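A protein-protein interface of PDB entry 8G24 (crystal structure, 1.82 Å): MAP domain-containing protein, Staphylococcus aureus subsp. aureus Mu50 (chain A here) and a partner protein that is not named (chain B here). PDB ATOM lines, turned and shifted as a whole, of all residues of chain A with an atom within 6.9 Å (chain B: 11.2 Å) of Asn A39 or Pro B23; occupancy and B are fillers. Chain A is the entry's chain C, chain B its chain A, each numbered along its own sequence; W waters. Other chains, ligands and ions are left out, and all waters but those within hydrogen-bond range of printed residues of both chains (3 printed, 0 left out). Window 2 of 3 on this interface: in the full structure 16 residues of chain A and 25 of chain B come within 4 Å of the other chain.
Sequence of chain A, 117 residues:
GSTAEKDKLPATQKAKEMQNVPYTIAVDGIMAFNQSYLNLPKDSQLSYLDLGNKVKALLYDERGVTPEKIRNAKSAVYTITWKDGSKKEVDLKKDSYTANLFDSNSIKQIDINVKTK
Water W2 lies within hydrogen-bond range of O of Asn A39 (2.6 Å) and O of Ala B24 (2.9 Å). Water W1 lies within hydrogen-bond range of the backbone carbonyl oxygen of Ser B22 and the side-chain amide nitrogen of Asn A39. Water W3 lies within hydrogen-bond range of the side-chain hydroxyl (OH) of Tyr A23 (2.9 Å), the backbone carbonyl oxygen (O) of Tyr A37 (3.1 Å) and the backbone carbonyl oxygen (O) of Gln B26 (3.2 Å).
The backbone carbonyl oxygen (O) of Met A18 lies within hydrogen-bond range of the side-chain amide nitrogen (ND2) of Asn A20 (3.4 Å). ND2 of Asn A20 is in hydrogen-bond range of OD1 of Asn A39 (2.8 Å). The backbone carbonyl oxygen of Val A21 lies within hydrogen-bond range of the backbone NH of Leu A38 (2.8 Å). The side-chain amide oxygen (OE1) of Gln B21 lies within hydrogen-bond range of the side-chain amide nitrogen (NE2) of Gln B26 (3.0 Å).
Printed residues of chain B that touch a printed residue of chain A: Pro B23, Ala B24, Gly B25, Gln B26 and Arg B28. Along chain B the printed residues that touch a printed residue of chain A span positions 23 to 28. Of the 11 printed residues of chain A, 4 touch a printed residue of chain B. Among the printed residues, 9 pairs touch across the chains.
OE1 of Gln B26 touches ND2 of Asn A20, at 3.6 Å. Tyr A37 touches Gly B25 (O to CA, 3.1 Å). Leu A38 touches Ala B24 (CD1 to O, 3.7 Å).
N of Tyr A37 sits at hydrogen-bond distance from O of Gln B26, 2.8 Å away. The side-chain hydroxyl of Tyr A37 sits close to the guanidinium group of Arg B28, 3.3 Å away. The side-chain amide nitrogen (ND2) of Asn A39 sits at hydrogen-bond distance from the backbone carbonyl oxygen (O) of Pro B23, at 3.3 Å. O of Ala B24 is in hydrogen-bond range of N of Asn A39, 3.0 Å away. ND2 of Asn A39 lies close to N of Gly B25, at 3.5 Å. OE1 of Gln B26 lies close to OD1 of Asn A39 (3.0 Å).
Asn A20 touches just one residue of chain B: Gln B26. Asn A39 touches just these residues of chain B: Pro B23 (3.3 Å), Ala B24 (3.0 Å), Gly B25 (3.5 Å) and Gln B26 (3.0 Å). Of chain A, only Asn A39 (3.3 Å) comes within 4 Å of Pro B23. Of the printed residues of chain A, Ala B24 touches Leu A38 and Asn A39. Printed residues of chain A within 4 Å of Gln B26: Asn A20, Tyr A37 and Asn A39. The nearest residue of chain B that does not touch Asn A39 is Ser B22 (4.03 Å).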
ATOM      1  N   MET A  18      19.615  27.428  10.555  1.00  0.00           N
ATOM      2  CA  MET A  18      20.028  26.071  10.873  1.00  0.00           C
ATOM      3  C   MET A  18      21.540  25.927  10.764  1.00  0.00           C
ATOM      4  O   MET A  18      22.186  26.580   9.941  1.00  0.00           O
ATOM      5  CB  MET A  18      19.311  25.053   9.970  1.00  0.00           C
ATOM      6  CG  MET A  18      17.825  24.886  10.327  1.00  0.00           C
ATOM      7  SD  MET A  18      17.055  23.319   9.838  1.00  0.00           S
ATOM      8  CE  MET A  18      16.244  22.802  11.349  1.00  0.00           C
ATOM      9  N   GLN A  19      22.084  25.128  11.672  1.00  0.00           N
ATOM     10  CA  GLN A  19      23.441  24.620  11.580  1.00  0.00           C
ATOM     11  C   GLN A  19      23.541  23.641  10.420  1.00  0.00           C
ATOM     12  O   GLN A  19      22.643  22.823  10.203  1.00  0.00           O
ATOM     13  CB  GLN A  19      23.808  23.914  12.887  1.00  0.00           C
ATOM     14  CG  GLN A  19      25.282  23.707  13.087  1.00  0.00           C
ATOM     15  CD  GLN A  19      25.988  24.989  13.464  1.00  0.00           C
ATOM     16  OE1 GLN A  19      26.109  25.324  14.644  1.00  0.00           O
ATOM     17  NE2 GLN A  19      26.458  25.719  12.461  1.00  0.00           N
ATOM     18  N   ASN A  20      24.648  23.704   9.692  1.00  0.00           N
ATOM     19  CA  ASN A  20      24.911  22.803   8.570  1.00  0.00           C
ATOM     20  C   ASN A  20      26.109  21.938   8.937  1.00  0.00           C
ATOM     21  O   ASN A  20      27.252  22.388   8.843  1.00  0.00           O
ATOM     22  CB  ASN A  20      25.164  23.592   7.289  1.00  0.00           C
ATOM     23  CG  ASN A  20      24.146  24.692   7.085  1.00  0.00           C
ATOM     24  OD1 ASN A  20      24.474  25.777   6.623  1.00  0.00           O
ATOM     25  ND2 ASN A  20      22.896  24.413   7.440  1.00  0.00           N
ATOM     26  N   VAL A  21      25.847  20.703   9.340  1.00  0.00           N
ATOM     27  CA  VAL A  21      26.860  19.799   9.876  1.00  0.00           C
ATOM     28  C   VAL A  21      27.317  18.876   8.759  1.00  0.00           C
ATOM     29  O   VAL A  21      26.486  18.136   8.206  1.00  0.00           O
ATOM     30  CB  VAL A  21      26.288  18.993  11.047  1.00  0.00           C
ATOM     31  CG1 VAL A  21      27.215  17.840  11.418  1.00  0.00           C
ATOM     32  CG2 VAL A  21      26.056  19.894  12.262  1.00  0.00           C
ATOM     33  N   TYR A  23      28.469  15.655   6.834  1.00  0.00           N
ATOM     34  CA  TYR A  23      28.342  14.233   7.121  1.00  0.00           C
ATOM     35  C   TYR A  23      28.821  13.432   5.915  1.00  0.00           C
ATOM     36  O   TYR A  23      28.826  13.909   4.774  1.00  0.00           O
ATOM     37  CB  TYR A  23      26.896  13.824   7.487  1.00  0.00           C
ATOM     38  CG  TYR A  23      25.973  13.807   6.299  1.00  0.00           C
ATOM     39  CD1 TYR A  23      25.831  12.659   5.543  1.00  0.00           C
ATOM     40  CD2 TYR A  23      25.226  14.938   5.938  1.00  0.00           C
ATOM     41  CE1 TYR A  23      24.969  12.630   4.430  1.00  0.00           C
ATOM     42  CE2 TYR A  23      24.379  14.909   4.852  1.00  0.00           C
ATOM     43  CZ  TYR A  23      24.260  13.749   4.106  1.00  0.00           C
ATOM     44  OH  TYR A  23      23.423  13.719   3.017  1.00  0.00           O
ATOM     45  N   TYR A  37      25.713  18.103   3.799  1.00  0.00           N
ATOM     46  CA  TYR A  37      25.491  18.666   5.112  1.00  0.00           C
ATOM     47  C   TYR A  37      24.071  18.384   5.589  1.00  0.00           C
ATOM     48  O   TYR A  37      23.103  18.418   4.819  1.00  0.00           O
ATOM     49  CB  TYR A  37      25.740  20.175   5.113  1.00  0.00           C
ATOM     50  CG  TYR A  37      27.043  20.599   4.486  1.00  0.00           C
ATOM     51  CD1 TYR A  37      27.176  20.649   3.102  1.00  0.00           C
ATOM     52  CD2 TYR A  37      28.130  20.956   5.261  1.00  0.00           C
ATOM     53  CE1 TYR A  37      28.356  21.034   2.511  1.00  0.00           C
ATOM     54  CE2 TYR A  37      29.323  21.349   4.674  1.00  0.00           C
ATOM     55  CZ  TYR A  37      29.432  21.389   3.312  1.00  0.00           C
ATOM     56  OH  TYR A  37      30.616  21.780   2.736  1.00  0.00           O
ATOM     57  N   LEU A  38      23.964  18.141   6.892  1.00  0.00           N
ATOM     58  CA  LEU A  38      22.700  17.895   7.564  1.00  0.00           C
ATOM     59  C   LEU A  38      22.311  19.135   8.354  1.00  0.00           C
ATOM     60  O   LEU A  38      23.128  19.680   9.105  1.00  0.00           O
ATOM     61  CB  LEU A  38      22.796  16.692   8.503  1.00  0.00           C
ATOM     62  CG  LEU A  38      21.520  16.344   9.268  1.00  0.00           C
ATOM     63  CD1 LEU A  38      20.562  15.627   8.330  1.00  0.00           C
ATOM     64  CD2 LEU A  38      21.866  15.506  10.480  1.00  0.00           C
ATOM     65  N   ASN A  39      21.076  19.584   8.175  1.00  0.00           N
ATOM     66  CA  ASN A  39      20.585  20.730   8.920  1.00  0.00           C
ATOM     67  C   ASN A  39      20.162  20.303  10.315  1.00  0.00           C
ATOM     68  O   ASN A  39      19.459  19.305  10.487  1.00  0.00           O
ATOM     69  CB  ASN A  39      19.397  21.370   8.218  1.00  0.00           C
ATOM     70  CG  ASN A  39      19.791  22.104   6.959  1.00  0.00           C
ATOM     71  OD1 ASN A  39      20.939  22.516   6.789  1.00  0.00           O
ATOM     72  ND2 ASN A  39      18.831  22.279   6.063  1.00  0.00           N
ATOM     73  N   LEU A  40      20.617  21.040  11.304  1.00  0.00           N
ATOM     74  CA  LEU A  40      20.077  20.934  12.647  1.00  0.00           C
ATOM     75  C   LEU A  40      19.611  22.312  13.106  1.00  0.00           C
ATOM     76  O   LEU A  40      20.233  23.315  12.754  1.00  0.00           O
ATOM     77  CB  LEU A  40      21.117  20.394  13.623  1.00  0.00           C
ATOM     78  CG  LEU A  40      21.569  18.955  13.388  1.00  0.00           C
ATOM     79  CD1 LEU A  40      22.605  18.614  14.443  1.00  0.00           C
ATOM     80  CD2 LEU A  40      20.408  17.994  13.425  1.00  0.00           C
ATOM     81  N   PRO A  41      18.523  22.408  13.864  1.00  0.00           N
ATOM     82  CA  PRO A  41      18.085  23.732  14.333  1.00  0.00           C
ATOM     83  C   PRO A  41      19.217  24.400  15.100  1.00  0.00           C
ATOM     84  O   PRO A  41      19.832  23.793  15.975  1.00  0.00           O
ATOM     85  CB  PRO A  41      16.882  23.418  15.236  1.00  0.00           C
ATOM     86  CG  PRO A  41      16.484  21.984  14.896  1.00  0.00           C
ATOM     87  CD  PRO A  41      17.757  21.309  14.471  1.00  0.00           C
ATOM     88  N   LYS A  54      17.343  11.017  12.771  1.00  0.00           N
ATOM     89  CA  LYS A  54      17.782  11.769  11.601  1.00  0.00           C
ATOM     90  C   LYS A  54      18.809  10.985  10.788  1.00  0.00           C
ATOM     91  O   LYS A  54      18.790  11.022   9.549  1.00  0.00           O
ATOM     92  CB  LYS A  54      18.389  13.101  12.013  1.00  0.00           C
ATOM     93  CG  LYS A  54      17.419  14.139  12.559  1.00  0.00           C
ATOM     94  CD  LYS A  54      18.263  15.203  13.212  1.00  0.00           C
ATOM     95  CE  LYS A  54      17.418  16.318  13.803  1.00  0.00           C
ATOM     96  NZ  LYS A  54      16.985  17.239  12.719  1.00  0.00           N
ATOM     97  N   ILE B  20      23.016  22.308  -4.040  1.00  0.00           N
ATOM     98  CA  ILE B  20      21.759  21.586  -3.936  1.00  0.00           C
ATOM     99  C   ILE B  20      21.201  21.795  -2.536  1.00  0.00           C
ATOM    100  O   ILE B  20      21.910  21.599  -1.545  1.00  0.00           O
ATOM    101  CB  ILE B  20      21.977  20.087  -4.217  1.00  0.00           C
ATOM    102  CG1 ILE B  20      22.554  19.881  -5.626  1.00  0.00           C
ATOM    103  CG2 ILE B  20      20.643  19.334  -4.065  1.00  0.00           C
ATOM    104  CD1 ILE B  20      24.020  19.442  -5.575  1.00  0.00           C
ATOM    105  N   GLN B  21      19.935  22.168  -2.450  1.00  0.00           N
ATOM    106  CA  GLN B  21      19.285  22.423  -1.177  1.00  0.00           C
ATOM    107  C   GLN B  21      17.975  21.646  -1.090  1.00  0.00           C
ATOM    108  O   GLN B  21      17.202  21.571  -2.054  1.00  0.00           O
ATOM    109  CB  GLN B  21      19.047  23.936  -0.982  1.00  0.00           C
ATOM    110  CG  GLN B  21      20.328  24.677  -0.654  1.00  0.00           C
ATOM    111  CD  GLN B  21      20.135  25.726   0.426  1.00  0.00           C
ATOM    112  OE1 GLN B  21      20.930  25.827   1.361  1.00  0.00           O
ATOM    113  NE2 GLN B  21      19.080  26.520   0.297  1.00  0.00           N
ATOM    114  N   SER B  22      17.735  21.073   0.081  1.00  0.00           N
ATOM    115  CA  SER B  22      16.515  20.365   0.423  1.00  0.00           C
ATOM    116  C   SER B  22      16.192  20.680   1.881  1.00  0.00           C
ATOM    117  O   SER B  22      17.083  21.055   2.650  1.00  0.00           O
ATOM    118  CB  SER B  22      16.666  18.849   0.252  1.00  0.00           C
ATOM    119  OG  SER B  22      17.181  18.512  -1.029  1.00  0.00           O
ATOM    120  N   PRO B  23      14.946  20.462   2.297  1.00  0.00           N
ATOM    121  CA  PRO B  23      14.588  20.796   3.685  1.00  0.00           C
ATOM    122  C   PRO B  23      15.529  20.187   4.707  1.00  0.00           C
ATOM    123  O   PRO B  23      15.852  20.832   5.694  1.00  0.00           O
ATOM    124  CB  PRO B  23      13.154  20.251   3.812  1.00  0.00           C
ATOM    125  CG  PRO B  23      12.598  20.353   2.408  1.00  0.00           C
ATOM    126  CD  PRO B  23      13.789  19.961   1.526  1.00  0.00           C
ATOM    127  N   ALA B  24      16.020  18.986   4.488  1.00  0.00           N
ATOM    128  CA  ALA B  24      16.809  18.311   5.512  1.00  0.00           C
ATOM    129  C   ALA B  24      18.293  18.654   5.447  1.00  0.00           C
ATOM    130  O   ALA B  24      19.010  18.392   6.414  1.00  0.00           O
ATOM    131  CB  ALA B  24      16.656  16.777   5.410  1.00  0.00           C
ATOM    132  N   GLY B  25      18.779  19.253   4.367  1.00  0.00           N
ATOM    133  CA  GLY B  25      20.206  19.480   4.268  1.00  0.00           C
ATOM    134  C   GLY B  25      20.600  19.951   2.883  1.00  0.00           C
ATOM    135  O   GLY B  25      19.751  20.211   2.022  1.00  0.00           O
ATOM    136  N   GLN B  26      21.916  20.027   2.677  1.00  0.00           N
ATOM    137  CA  GLN B  26      22.442  20.486   1.406  1.00  0.00           C
ATOM    138  C   GLN B  26      23.538  19.574   0.895  1.00  0.00           C
ATOM    139  O   GLN B  26      24.095  18.739   1.618  1.00  0.00           O
ATOM    140  CB  GLN B  26      23.032  21.896   1.486  1.00  0.00           C
ATOM    141  CG  GLN B  26      22.112  22.926   1.982  1.00  0.00           C
ATOM    142  CD  GLN B  26      22.499  23.407   3.353  1.00  0.00           C
ATOM    143  OE1 GLN B  26      22.660  22.615   4.276  1.00  0.00           O
ATOM    144  NE2 GLN B  26      22.710  24.716   3.482  1.00  0.00           N
ATOM    145  N   SER B  27      23.879  19.811  -0.368  1.00  0.00           N
ATOM    146  CA  SER B  27      24.969  19.100  -1.011  1.00  0.00           C
ATOM    147  C   SER B  27      25.667  20.036  -1.985  1.00  0.00           C
ATOM    148  O   SER B  27      25.071  20.981  -2.485  1.00  0.00           O
ATOM    149  CB  SER B  27      24.498  17.853  -1.780  1.00  0.00           C
ATOM    150  OG  SER B  27      24.188  16.802  -0.896  1.00  0.00           O
ATOM    151  N   ARG B  28      26.924  19.762  -2.264  1.00  0.00           N
ATOM    152  CA  ARG B  28      27.651  20.432  -3.326  1.00  0.00           C
ATOM    153  C   ARG B  28      28.233  19.381  -4.255  1.00  0.00           C
ATOM    154  O   ARG B  28      28.795  18.370  -3.813  1.00  0.00           O
ATOM    155  CB  ARG B  28      28.760  21.295  -2.765  1.00  0.00           C
ATOM    156  CG  ARG B  28      28.258  22.296  -1.752  1.00  0.00           C
ATOM    157  CD  ARG B  28      29.451  22.904  -1.037  1.00  0.00           C
ATOM    158  NE  ARG B  28      29.056  23.730   0.091  1.00  0.00           N
ATOM    159  CZ  ARG B  28      29.911  24.380   0.859  1.00  0.00           C
ATOM    160  NH1 ARG B  28      31.216  24.312   0.644  1.00  0.00           N
ATOM    161  NH2 ARG B  28      29.444  25.113   1.865  1.00  0.00           N
ATOM    162  N   TRP B  46      21.031  14.789  -6.722  1.00  0.00           N
ATOM    163  CA  TRP B  46      19.683  15.325  -6.822  1.00  0.00           C
ATOM    164  C   TRP B  46      19.231  15.919  -5.482  1.00  0.00           C
ATOM    165  O   TRP B  46      19.672  15.523  -4.392  1.00  0.00           O
ATOM    166  CB  TRP B  46      18.739  14.209  -7.314  1.00  0.00           C
ATOM    167  CG  TRP B  46      17.305  14.643  -7.424  1.00  0.00           C
ATOM    168  CD1 TRP B  46      16.691  15.139  -8.521  1.00  0.00           C
ATOM    169  CD2 TRP B  46      16.320  14.585  -6.401  1.00  0.00           C
ATOM    170  NE1 TRP B  46      15.376  15.418  -8.252  1.00  0.00           N
ATOM    171  CE2 TRP B  46      15.126  15.074  -6.948  1.00  0.00           C
ATOM    172  CE3 TRP B  46      16.325  14.150  -5.077  1.00  0.00           C
ATOM    173  CZ2 TRP B  46      13.950  15.150  -6.210  1.00  0.00           C
ATOM    174  CZ3 TRP B  46      15.159  14.223  -4.340  1.00  0.00           C
ATOM    175  CH2 TRP B  46      13.989  14.720  -4.905  1.00  0.00           C
ATOM    176  N   GLY B  47      18.335  16.888  -5.576  1.00  0.00           N
ATOM    177  CA  GLY B  47      17.734  17.491  -4.403  1.00  0.00           C
ATOM    178  C   GLY B  47      16.608  18.400  -4.842  1.00  0.00           C
ATOM    179  O   GLY B  47      16.298  18.520  -6.033  1.00  0.00           O
ATOM    180  N   SER B  48      15.992  19.038  -3.848  1.00  0.00           N
ATOM    181  CA  SER B  48      14.765  19.793  -4.096  1.00  0.00           C
ATOM    182  C   SER B  48      15.011  21.013  -4.977  1.00  0.00           C
ATOM    183  O   SER B  48      14.175  21.355  -5.828  1.00  0.00           O
ATOM    184  CB  SER B  48      14.149  20.252  -2.777  1.00  0.00           C
ATOM    185  OG  SER B  48      13.850  19.179  -1.920  1.00  0.00           O
ATOM    186  N   ASN B  49      16.126  21.710  -4.767  1.00  0.00           N
ATOM    187  CA  ASN B  49      16.424  22.919  -5.529  1.00  0.00           C
ATOM    188  C   ASN B  49      17.895  22.901  -5.885  1.00  0.00           C
ATOM    189  O   ASN B  49      18.731  22.620  -5.021  1.00  0.00           O
ATOM    190  CB  ASN B  49      16.098  24.188  -4.731  1.00  0.00           C
ATOM    191  CG  ASN B  49      14.619  24.325  -4.417  1.00  0.00           C
ATOM    192  OD1 ASN B  49      13.812  24.639  -5.294  1.00  0.00           O
ATOM    193  ND2 ASN B  49      14.258  24.088  -3.162  1.00  0.00           N
ATOM    194  N   ILE B  50      18.214  23.176  -7.145  1.00  0.00           N
ATOM    195  CA  ILE B  50      19.582  23.075  -7.629  1.00  0.00           C
ATOM    196  C   ILE B  50      19.942  24.397  -8.289  1.00  0.00           C
ATOM    197  O   ILE B  50      19.283  24.815  -9.248  1.00  0.00           O
ATOM    198  CB  ILE B  50      19.767  21.898  -8.609  1.00  0.00           C
ATOM    199  CG1 ILE B  50      19.462  20.580  -7.889  1.00  0.00           C
ATOM    200  CG2 ILE B  50      21.171  21.891  -9.190  1.00  0.00           C
ATOM    201  CD1 ILE B  50      19.830  19.324  -8.672  1.00  0.00           C
HETATM  202  O   HOH W   1      18.571  23.541   2.897  1.00  0.00           O
HETATM  203  O   HOH W   2      17.954  17.820   9.008  1.00  0.00           O
HETATM  204  O   HOH W   3      22.226  16.366   2.685  1.00  0.00           O
